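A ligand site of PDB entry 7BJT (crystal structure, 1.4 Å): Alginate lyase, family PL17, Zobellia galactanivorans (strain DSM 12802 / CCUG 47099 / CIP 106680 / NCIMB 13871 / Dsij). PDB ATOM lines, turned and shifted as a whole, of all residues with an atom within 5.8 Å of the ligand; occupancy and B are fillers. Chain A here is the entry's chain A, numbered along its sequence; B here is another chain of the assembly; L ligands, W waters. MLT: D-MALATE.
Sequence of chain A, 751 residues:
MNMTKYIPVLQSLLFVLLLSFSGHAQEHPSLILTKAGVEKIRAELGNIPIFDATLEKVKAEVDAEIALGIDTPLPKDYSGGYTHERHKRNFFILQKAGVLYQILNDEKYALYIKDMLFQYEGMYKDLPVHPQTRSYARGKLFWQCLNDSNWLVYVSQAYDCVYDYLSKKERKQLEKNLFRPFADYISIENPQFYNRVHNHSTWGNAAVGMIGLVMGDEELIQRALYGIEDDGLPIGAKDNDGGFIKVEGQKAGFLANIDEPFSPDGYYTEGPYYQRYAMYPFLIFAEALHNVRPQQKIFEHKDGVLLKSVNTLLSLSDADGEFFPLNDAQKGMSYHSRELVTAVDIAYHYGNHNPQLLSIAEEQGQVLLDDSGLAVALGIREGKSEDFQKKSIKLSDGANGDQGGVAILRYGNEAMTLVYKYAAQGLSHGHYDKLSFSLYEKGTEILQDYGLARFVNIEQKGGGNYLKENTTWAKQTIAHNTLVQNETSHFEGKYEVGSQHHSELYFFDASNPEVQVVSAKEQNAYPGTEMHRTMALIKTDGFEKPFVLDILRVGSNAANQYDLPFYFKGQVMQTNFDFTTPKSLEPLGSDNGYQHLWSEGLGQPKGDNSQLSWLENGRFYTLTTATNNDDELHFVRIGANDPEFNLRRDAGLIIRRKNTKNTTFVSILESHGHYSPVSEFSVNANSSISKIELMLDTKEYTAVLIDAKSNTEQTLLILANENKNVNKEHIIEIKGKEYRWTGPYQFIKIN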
ATOM      1  N   SER A  79      18.352 -18.744 -10.643  1.00  0.00           N
ATOM      2  CA  SER A  79      17.652 -17.584 -11.164  1.00  0.00           C
ATOM      3  C   SER A  79      17.548 -16.435 -10.163  1.00  0.00           C
ATOM      4  O   SER A  79      17.390 -16.658  -8.954  1.00  0.00           O
ATOM      5  CB  SER A  79      16.276 -17.963 -11.709  1.00  0.00           C
ATOM      6  OG  SER A  79      15.366 -18.345 -10.692  1.00  0.00           O
ATOM      7  N   HIS A  84      23.269 -16.014 -13.461  1.00  0.00           N
ATOM      8  CA  HIS A  84      22.070 -16.315 -14.224  1.00  0.00           C
ATOM      9  C   HIS A  84      21.574 -15.044 -14.924  1.00  0.00           C
ATOM     10  O   HIS A  84      21.353 -15.027 -16.146  1.00  0.00           O
ATOM     11  CB  HIS A  84      20.986 -16.856 -13.302  1.00  0.00           C
ATOM     12  CG  HIS A  84      19.770 -17.332 -14.026  1.00  0.00           C
ATOM     13  ND1 HIS A  84      19.564 -18.660 -14.327  1.00  0.00           N
ATOM     14  CD2 HIS A  84      18.676 -16.664 -14.486  1.00  0.00           C
ATOM     15  CE1 HIS A  84      18.396 -18.794 -14.945  1.00  0.00           C
ATOM     16  NE2 HIS A  84      17.845 -17.596 -15.057  1.00  0.00           N
ATOM     17  N   LYS A  88      21.720 -14.230 -18.962  1.00  0.00           N
ATOM     18  CA  LYS A  88      20.399 -14.011 -19.525  1.00  0.00           C
ATOM     19  C   LYS A  88      20.300 -12.645 -20.201  1.00  0.00           C
ATOM     20  O   LYS A  88      19.879 -12.530 -21.363  1.00  0.00           O
ATOM     21  CB  LYS A  88      19.334 -14.154 -18.431  1.00  0.00           C
ATOM     22  CG  LYS A  88      17.899 -13.980 -18.898  1.00  0.00           C
ATOM     23  CD  LYS A  88      16.921 -14.432 -17.815  1.00  0.00           C
ATOM     24  CE  LYS A  88      15.481 -14.218 -18.217  1.00  0.00           C
ATOM     25  NZ  LYS A  88      14.557 -14.750 -17.175  1.00  0.00           N
ATOM     26  N   TRP A 143      21.880 -23.104 -14.819  1.00  0.00           N
ATOM     27  CA  TRP A 143      21.609 -24.266 -13.985  1.00  0.00           C
ATOM     28  C   TRP A 143      20.878 -25.378 -14.748  1.00  0.00           C
ATOM     29  O   TRP A 143      20.982 -26.529 -14.362  1.00  0.00           O
ATOM     30  CB  TRP A 143      20.820 -23.862 -12.733  1.00  0.00           C
ATOM     31  CG  TRP A 143      19.370 -23.556 -12.971  1.00  0.00           C
ATOM     32  CD1 TRP A 143      18.827 -22.417 -13.520  1.00  0.00           C
ATOM     33  CD2 TRP A 143      18.257 -24.400 -12.655  1.00  0.00           C
ATOM     34  NE1 TRP A 143      17.460 -22.523 -13.581  1.00  0.00           N
ATOM     35  CE2 TRP A 143      17.091 -23.724 -13.046  1.00  0.00           C
ATOM     36  CE3 TRP A 143      18.140 -25.664 -12.065  1.00  0.00           C
ATOM     37  CZ2 TRP A 143      15.812 -24.275 -12.871  1.00  0.00           C
ATOM     38  CZ3 TRP A 143      16.897 -26.217 -11.902  1.00  0.00           C
ATOM     39  CH2 TRP A 143      15.736 -25.521 -12.314  1.00  0.00           C
ATOM     40  N   GLN A 144      20.176 -25.036 -15.818  1.00  0.00           N
ATOM     41  CA  GLN A 144      19.416 -26.019 -16.587  1.00  0.00           C
ATOM     42  C   GLN A 144      19.584 -25.781 -18.074  1.00  0.00           C
ATOM     43  O   GLN A 144      19.735 -24.644 -18.528  1.00  0.00           O
ATOM     44  CB  GLN A 144      17.930 -25.970 -16.188  1.00  0.00           C
ATOM     45  CG  GLN A 144      17.256 -24.612 -16.408  1.00  0.00           C
ATOM     46  CD  GLN A 144      15.760 -24.601 -16.116  1.00  0.00           C
ATOM     47  OE1 GLN A 144      15.133 -25.647 -15.983  1.00  0.00           O
ATOM     48  NE2 GLN A 144      15.188 -23.419 -16.021  1.00  0.00           N
ATOM     49  N   LEU A 146      17.357 -25.810 -20.301  1.00  0.00           N
ATOM     50  CA  LEU A 146      16.333 -24.911 -20.823  1.00  0.00           C
ATOM     51  C   LEU A 146      16.901 -23.505 -21.057  1.00  0.00           C
ATOM     52  O   LEU A 146      16.642 -22.889 -22.082  1.00  0.00           O
ATOM     53  CB  LEU A 146      15.149 -24.804 -19.860  1.00  0.00           C
ATOM     54  CG  LEU A 146      14.146 -23.695 -20.179  1.00  0.00           C
ATOM     55  CD1 LEU A 146      13.490 -23.911 -21.523  1.00  0.00           C
ATOM     56  CD2 LEU A 146      13.136 -23.616 -19.061  1.00  0.00           C
ATOM     57  N   ASN A 147      17.649 -23.000 -20.079  1.00  0.00           N
ATOM     58  CA  ASN A 147      18.156 -21.640 -20.174  1.00  0.00           C
ATOM     59  C   ASN A 147      19.332 -21.524 -21.147  1.00  0.00           C
ATOM     60  O   ASN A 147      19.426 -20.543 -21.870  1.00  0.00           O
ATOM     61  CB  ASN A 147      18.477 -21.092 -18.792  1.00  0.00           C
ATOM     62  CG  ASN A 147      17.240 -20.940 -17.928  1.00  0.00           C
ATOM     63  OD1 ASN A 147      16.187 -20.436 -18.383  1.00  0.00           O
ATOM     64  ND2 ASN A 147      17.339 -21.340 -16.701  1.00  0.00           N
ATOM     65  N   ASN A 150      17.448 -21.148 -24.297  1.00  0.00           N
ATOM     66  CA  ASN A 150      16.998 -19.757 -24.458  1.00  0.00           C
ATOM     67  C   ASN A 150      18.122 -18.935 -25.088  1.00  0.00           C
ATOM     68  O   ASN A 150      17.929 -18.209 -26.063  1.00  0.00           O
ATOM     69  CB  ASN A 150      16.662 -19.059 -23.131  1.00  0.00           C
ATOM     70  CG  ASN A 150      15.515 -19.682 -22.340  1.00  0.00           C
ATOM     71  OD1 ASN A 150      14.540 -20.283 -22.874  1.00  0.00           O
ATOM     72  ND2 ASN A 150      15.604 -19.514 -21.047  1.00  0.00           N
ATOM     73  N   ASN A 199       7.606 -28.028 -23.116  1.00  0.00           N
ATOM     74  CA  ASN A 199       8.150 -26.705 -23.444  1.00  0.00           C
ATOM     75  C   ASN A 199       9.688 -26.670 -23.474  1.00  0.00           C
ATOM     76  O   ASN A 199      10.268 -25.935 -24.245  1.00  0.00           O
ATOM     77  CB  ASN A 199       7.553 -25.593 -22.553  1.00  0.00           C
ATOM     78  CG  ASN A 199       8.021 -25.637 -21.107  1.00  0.00           C
ATOM     79  OD1 ASN A 199       7.362 -26.213 -20.237  1.00  0.00           O
ATOM     80  ND2 ASN A 199       9.160 -25.035 -20.836  1.00  0.00           N
ATOM     81  N   HIS A 200      10.331 -27.466 -22.629  1.00  0.00           N
ATOM     82  CA  HIS A 200      11.773 -27.605 -22.629  1.00  0.00           C
ATOM     83  C   HIS A 200      12.291 -28.020 -23.990  1.00  0.00           C
ATOM     84  O   HIS A 200      13.221 -27.427 -24.509  1.00  0.00           O
ATOM     85  CB  HIS A 200      12.249 -28.636 -21.603  1.00  0.00           C
ATOM     86  CG  HIS A 200      12.287 -28.128 -20.201  1.00  0.00           C
ATOM     87  ND1 HIS A 200      12.981 -28.760 -19.198  1.00  0.00           N
ATOM     88  CD2 HIS A 200      11.731 -27.036 -19.644  1.00  0.00           C
ATOM     89  CE1 HIS A 200      12.841 -28.075 -18.070  1.00  0.00           C
ATOM     90  NE2 HIS A 200      12.080 -27.025 -18.324  1.00  0.00           N
ATOM     91  N   TYR A 273      -0.091 -20.178 -19.055  1.00  0.00           N
ATOM     92  CA  TYR A 273       1.173 -19.617 -18.574  1.00  0.00           C
ATOM     93  C   TYR A 273       2.345 -20.239 -19.332  1.00  0.00           C
ATOM     94  O   TYR A 273       3.271 -19.549 -19.772  1.00  0.00           O
ATOM     95  CB  TYR A 273       1.302 -19.799 -17.067  1.00  0.00           C
ATOM     96  CG  TYR A 273       2.626 -19.349 -16.487  1.00  0.00           C
ATOM     97  CD1 TYR A 273       2.849 -18.016 -16.167  1.00  0.00           C
ATOM     98  CD2 TYR A 273       3.642 -20.269 -16.224  1.00  0.00           C
ATOM     99  CE1 TYR A 273       4.066 -17.599 -15.635  1.00  0.00           C
ATOM    100  CE2 TYR A 273       4.857 -19.861 -15.682  1.00  0.00           C
ATOM    101  CZ  TYR A 273       5.053 -18.526 -15.396  1.00  0.00           C
ATOM    102  OH  TYR A 273       6.274 -18.149 -14.862  1.00  0.00           O
ATOM    103  N   TYR A 274       2.308 -21.571 -19.476  1.00  0.00           N
ATOM    104  CA  TYR A 274       3.338 -22.264 -20.238  1.00  0.00           C
ATOM    105  C   TYR A 274       3.159 -22.155 -21.748  1.00  0.00           C
ATOM    106  O   TYR A 274       4.141 -22.170 -22.479  1.00  0.00           O
ATOM    107  CB  TYR A 274       3.539 -23.720 -19.748  1.00  0.00           C
ATOM    108  CG  TYR A 274       4.497 -23.725 -18.574  1.00  0.00           C
ATOM    109  CD1 TYR A 274       5.844 -23.492 -18.792  1.00  0.00           C
ATOM    110  CD2 TYR A 274       4.044 -23.880 -17.268  1.00  0.00           C
ATOM    111  CE1 TYR A 274       6.736 -23.430 -17.750  1.00  0.00           C
ATOM    112  CE2 TYR A 274       4.940 -23.829 -16.194  1.00  0.00           C
ATOM    113  CZ  TYR A 274       6.287 -23.609 -16.445  1.00  0.00           C
ATOM    114  OH  TYR A 274       7.183 -23.552 -15.396  1.00  0.00           O
ATOM    115  N   ARG A 276       2.233 -19.364 -23.182  1.00  0.00           N
ATOM    116  CA  ARG A 276       2.954 -18.100 -23.332  1.00  0.00           C
ATOM    117  C   ARG A 276       4.456 -18.311 -23.494  1.00  0.00           C
ATOM    118  O   ARG A 276       5.065 -17.748 -24.389  1.00  0.00           O
ATOM    119  CB  ARG A 276       2.629 -17.187 -22.127  1.00  0.00           C
ATOM    120  CG  ARG A 276       3.491 -15.948 -21.910  1.00  0.00           C
ATOM    121  CD  ARG A 276       4.857 -16.190 -21.298  1.00  0.00           C
ATOM    122  NE  ARG A 276       4.864 -17.115 -20.162  1.00  0.00           N
ATOM    123  CZ  ARG A 276       5.933 -17.375 -19.416  1.00  0.00           C
ATOM    124  NH1 ARG A 276       7.089 -16.760 -19.631  1.00  0.00           N
ATOM    125  NH2 ARG A 276       5.845 -18.256 -18.431  1.00  0.00           N
ATOM    126  N   TYR A 277       5.026 -19.161 -22.639  1.00  0.00           N
ATOM    127  CA  TYR A 277       6.464 -19.411 -22.656  1.00  0.00           C
ATOM    128  C   TYR A 277       6.913 -20.074 -23.951  1.00  0.00           C
ATOM    129  O   TYR A 277       7.897 -19.655 -24.561  1.00  0.00           O
ATOM    130  CB  TYR A 277       6.867 -20.253 -21.450  1.00  0.00           C
ATOM    131  CG  TYR A 277       8.357 -20.390 -21.231  1.00  0.00           C
ATOM    132  CD1 TYR A 277       9.171 -19.275 -21.153  1.00  0.00           C
ATOM    133  CD2 TYR A 277       8.938 -21.631 -21.083  1.00  0.00           C
ATOM    134  CE1 TYR A 277      10.535 -19.384 -20.949  1.00  0.00           C
ATOM    135  CE2 TYR A 277      10.308 -21.772 -20.888  1.00  0.00           C
ATOM    136  CZ  TYR A 277      11.106 -20.635 -20.812  1.00  0.00           C
ATOM    137  OH  TYR A 277      12.467 -20.747 -20.622  1.00  0.00           O
ATOM    138  N   HIS A 429       3.192 -30.009 -15.322  1.00  0.00           N
ATOM    139  CA  HIS A 429       2.701 -28.815 -14.624  1.00  0.00           C
ATOM    140  C   HIS A 429       1.212 -28.881 -14.284  1.00  0.00           C
ATOM    141  O   HIS A 429       0.701 -27.958 -13.648  1.00  0.00           O
ATOM    142  CB  HIS A 429       3.025 -27.576 -15.441  1.00  0.00           C
ATOM    143  CG  HIS A 429       4.488 -27.302 -15.532  1.00  0.00           C
ATOM    144  ND1 HIS A 429       5.227 -26.938 -14.423  1.00  0.00           N
ATOM    145  CD2 HIS A 429       5.361 -27.393 -16.559  1.00  0.00           C
ATOM    146  CE1 HIS A 429       6.483 -26.799 -14.772  1.00  0.00           C
ATOM    147  NE2 HIS A 429       6.601 -27.060 -16.061  1.00  0.00           N
ATOM    148  N   ARG A 454       5.640 -20.599  -6.164  1.00  0.00           N
ATOM    149  CA  ARG A 454       6.934 -20.295  -6.774  1.00  0.00           C
ATOM    150  C   ARG A 454       6.939 -18.796  -7.014  1.00  0.00           C
ATOM    151  O   ARG A 454       5.914 -18.227  -7.401  1.00  0.00           O
ATOM    152  CB  ARG A 454       7.073 -21.009  -8.117  1.00  0.00           C
ATOM    153  CG  ARG A 454       8.367 -20.706  -8.874  1.00  0.00           C
ATOM    154  CD  ARG A 454       8.457 -21.503 -10.159  1.00  0.00           C
ATOM    155  NE  ARG A 454       9.624 -21.067 -10.943  1.00  0.00           N
ATOM    156  CZ  ARG A 454       9.688 -21.019 -12.271  1.00  0.00           C
ATOM    157  NH1 ARG A 454       8.662 -21.385 -13.031  1.00  0.00           N
ATOM    158  NH2 ARG A 454      10.794 -20.577 -12.848  1.00  0.00           N
ATOM    159  N   VAL A 456       8.763 -16.554  -9.378  1.00  0.00           N
ATOM    160  CA  VAL A 456       9.520 -16.955 -10.567  1.00  0.00           C
ATOM    161  C   VAL A 456      10.734 -16.045 -10.746  1.00  0.00           C
ATOM    162  O   VAL A 456      10.606 -14.827 -10.880  1.00  0.00           O
ATOM    163  CB  VAL A 456       8.631 -16.945 -11.826  1.00  0.00           C
ATOM    164  CG1 VAL A 456       9.450 -17.228 -13.076  1.00  0.00           C
ATOM    165  CG2 VAL A 456       7.503 -17.972 -11.676  1.00  0.00           C
ATOM    166  N   ASN A 457      11.921 -16.649 -10.745  1.00  0.00           N
ATOM    167  CA  ASN A 457      13.195 -15.938 -10.900  1.00  0.00           C
ATOM    168  C   ASN A 457      13.556 -15.007  -9.729  1.00  0.00           C
ATOM    169  O   ASN A 457      14.437 -14.156  -9.891  1.00  0.00           O
ATOM    170  CB  ASN A 457      13.297 -15.172 -12.235  1.00  0.00           C
ATOM    171  CG  ASN A 457      13.074 -16.033 -13.452  1.00  0.00           C
ATOM    172  OD1 ASN A 457      13.494 -17.205 -13.488  1.00  0.00           O
ATOM    173  ND2 ASN A 457      12.466 -15.464 -14.483  1.00  0.00           N
ATOM    174  N   GLY A 464      14.304 -19.069  -6.999  1.00  0.00           N
ATOM    175  CA  GLY A 464      13.301 -18.757  -8.005  1.00  0.00           C
ATOM    176  C   GLY A 464      12.648 -19.955  -8.642  1.00  0.00           C
ATOM    177  O   GLY A 464      11.960 -19.815  -9.642  1.00  0.00           O
ATOM    178  N   TYR A 466      10.565 -24.006  -8.383  1.00  0.00           N
ATOM    179  CA  TYR A 466       9.353 -24.567  -7.767  1.00  0.00           C
ATOM    180  C   TYR A 466       9.608 -24.938  -6.315  1.00  0.00           C
ATOM    181  O   TYR A 466      10.598 -25.577  -5.993  1.00  0.00           O
ATOM    182  CB  TYR A 466       8.798 -25.766  -8.567  1.00  0.00           C
ATOM    183  CG  TYR A 466       8.037 -25.280  -9.774  1.00  0.00           C
ATOM    184  CD1 TYR A 466       6.739 -24.795  -9.639  1.00  0.00           C
ATOM    185  CD2 TYR A 466       8.633 -25.199 -11.034  1.00  0.00           C
ATOM    186  CE1 TYR A 466       6.052 -24.284 -10.723  1.00  0.00           C
ATOM    187  CE2 TYR A 466       7.946 -24.687 -12.118  1.00  0.00           C
ATOM    188  CZ  TYR A 466       6.656 -24.237 -11.954  1.00  0.00           C
ATOM    189  OH  TYR A 466       5.984 -23.704 -13.024  1.00  0.00           O
ATOM    190  N   GLU B 680       9.352 -10.952 -15.538  1.00  0.00           N
ATOM    191  CA  GLU B 680       9.924 -11.932 -14.607  1.00  0.00           C
ATOM    192  C   GLU B 680      11.407 -11.655 -14.297  1.00  0.00           C
ATOM    193  O   GLU B 680      12.180 -12.581 -14.052  1.00  0.00           O
ATOM    194  CB  GLU B 680       9.673 -13.368 -15.080  1.00  0.00           C
ATOM    195  CG  GLU B 680       8.180 -13.642 -15.301  1.00  0.00           C
ATOM    196  CD  GLU B 680       7.853 -15.096 -15.543  1.00  0.00           C
ATOM    197  OE1 GLU B 680       8.579 -15.726 -16.324  1.00  0.00           O
ATOM    198  OE2 GLU B 680       6.845 -15.578 -14.950  1.00  0.00           O
HETATM  199  C1  MLT L   1      12.875 -19.620 -17.207  1.00  0.00           C
HETATM  200  O1  MLT L   1      12.760 -19.141 -18.354  1.00  0.00           O
HETATM  201  O2  MLT L   1      13.979 -19.755 -16.659  1.00  0.00           O
HETATM  202  C2  MLT L   1      11.660 -20.048 -16.438  1.00  0.00           C
HETATM  203  O3  MLT L   1      12.091 -20.825 -15.313  1.00  0.00           O
HETATM  204  C3  MLT L   1      10.701 -20.864 -17.297  1.00  0.00           C
HETATM  205  C4  MLT L   1       9.628 -21.438 -16.413  1.00  0.00           C
HETATM  206  O4  MLT L   1       9.483 -22.672 -16.334  1.00  0.00           O
HETATM  207  O5  MLT L   1       8.918 -20.651 -15.747  1.00  0.00           O
HETATM  208  O   HOH W   1      15.123 -17.347 -15.878  1.00  0.00           O
HETATM  209  O   HOH W   2      11.925 -16.251 -20.026  1.00  0.00           O
HETATM  210  O   HOH W   3      15.301 -20.734 -14.256  1.00  0.00           O
HETATM  211  O   HOH W   4       8.404 -18.274 -17.198  1.00  0.00           O
HETATM  212  O   HOH W   5      10.038 -24.710 -18.190  1.00  0.00           O
HETATM  213  O   HOH W   6      13.491 -19.709 -12.365  1.00  0.00           O
HETATM  214  O   HOH W   7      14.509 -17.179 -19.265  1.00  0.00           O
HETATM  215  O   HOH W   8      11.521 -16.632 -16.939  1.00  0.00           O
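Water W1 lies within hydrogen-bond range of an oxygen (O2) of the ligand, a ring nitrogen (NE2) of His 84, the side-chain amide oxygen (OD1) of Asn 457 and the side-chain amino group (NZ) of Lys 88.
Water W7 lies within hydrogen-bond range of O1 of the ligand, ND2 of Asn 150 and NZ of Lys 88.
Water W5 lies within hydrogen-bond range of ND2 of Asn 199 (2.8 Å), O4 of the ligand (2.8 Å) and NE2 of His 200 (3.1 Å).
Water W4 lies within hydrogen-bond range of the side-chain carboxylate (OE1) of Glu 680 of chain B, an oxygen (O5) of the ligand, the guanidinium group (NH2) of Arg 276 and the side-chain hydroxyl (OH) of Tyr 273.
Water W8 lies within hydrogen-bond range of the side-chain amide nitrogen (ND2) of Asn 457 (2.9 Å), an oxygen (O1) of the ligand (3.1 Å) and the side-chain carboxylate (OE1) of Glu 680 of chain B (3.1 Å).
Water W6 lies within hydrogen-bond range of OD1 of Asn 457 (2.7 Å), OG of Ser 79 (2.9 Å), NH2 of Arg 454 (2.9 Å), O of Gly 464 (3.1 Å) and O3 of the ligand (3.4 Å).
OH of Tyr 277 sits at hydrogen-bond distance from O1 of the ligand.
OH of Tyr 274 sits at hydrogen-bond distance from O4 of the ligand (2.6 Å).
The side-chain amide oxygen of Asn 147 sits close to an oxygen (O2) of the ligand, at 2.9 Å.
O5 of the ligand is in salt-bridge range of NH1 of Arg 454 (2.8 Å).
Gln 144 touches the ligand.
ND2 of Asn 150 touches O1 of the ligand, 3.9 Å away.
OH of Tyr 273 touches O5 of the ligand, 3.7 Å away.
Hydrophobic or aromatic side chains that line the ligand: Tyr 274 and Tyr 277.
Within 4 Å of the ligand: Gln 144, Asn 147, Asn 150, Tyr 273, Tyr 274, Tyr 277 and Arg 454.
The side-chain amide oxygen (OD1) of Asn 150 sits close to the backbone carbonyl oxygen (O) of Leu 146.
OH of Tyr 274 sits at hydrogen-bond distance from OH of Tyr 466 (2.7 Å).
The side-chain amide nitrogen (NE2) of Gln 144 lies close to the side-chain amide nitrogen (ND2) of Asn 147.
The side-chain amide nitrogen (ND2) of Asn 147 lies close to the indole nitrogen (NE1) of Trp 143, at 3.3 Å.
The side-chain carboxylate of Glu 680 of chain B sits at hydrogen-bond distance from the side-chain hydroxyl of Tyr 273, at 2.6 Å.
The side-chain amide oxygen (OD1) of Asn 147 is in hydrogen-bond range of the side-chain amide nitrogen (ND2) of Asn 150, 2.9 Å away.
OH of Tyr 277 sits at hydrogen-bond distance from OD1 of Asn 150 (3.1 Å).
NE of Arg 454 sits at hydrogen-bond distance from O of Gly 464, 3.0 Å away.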
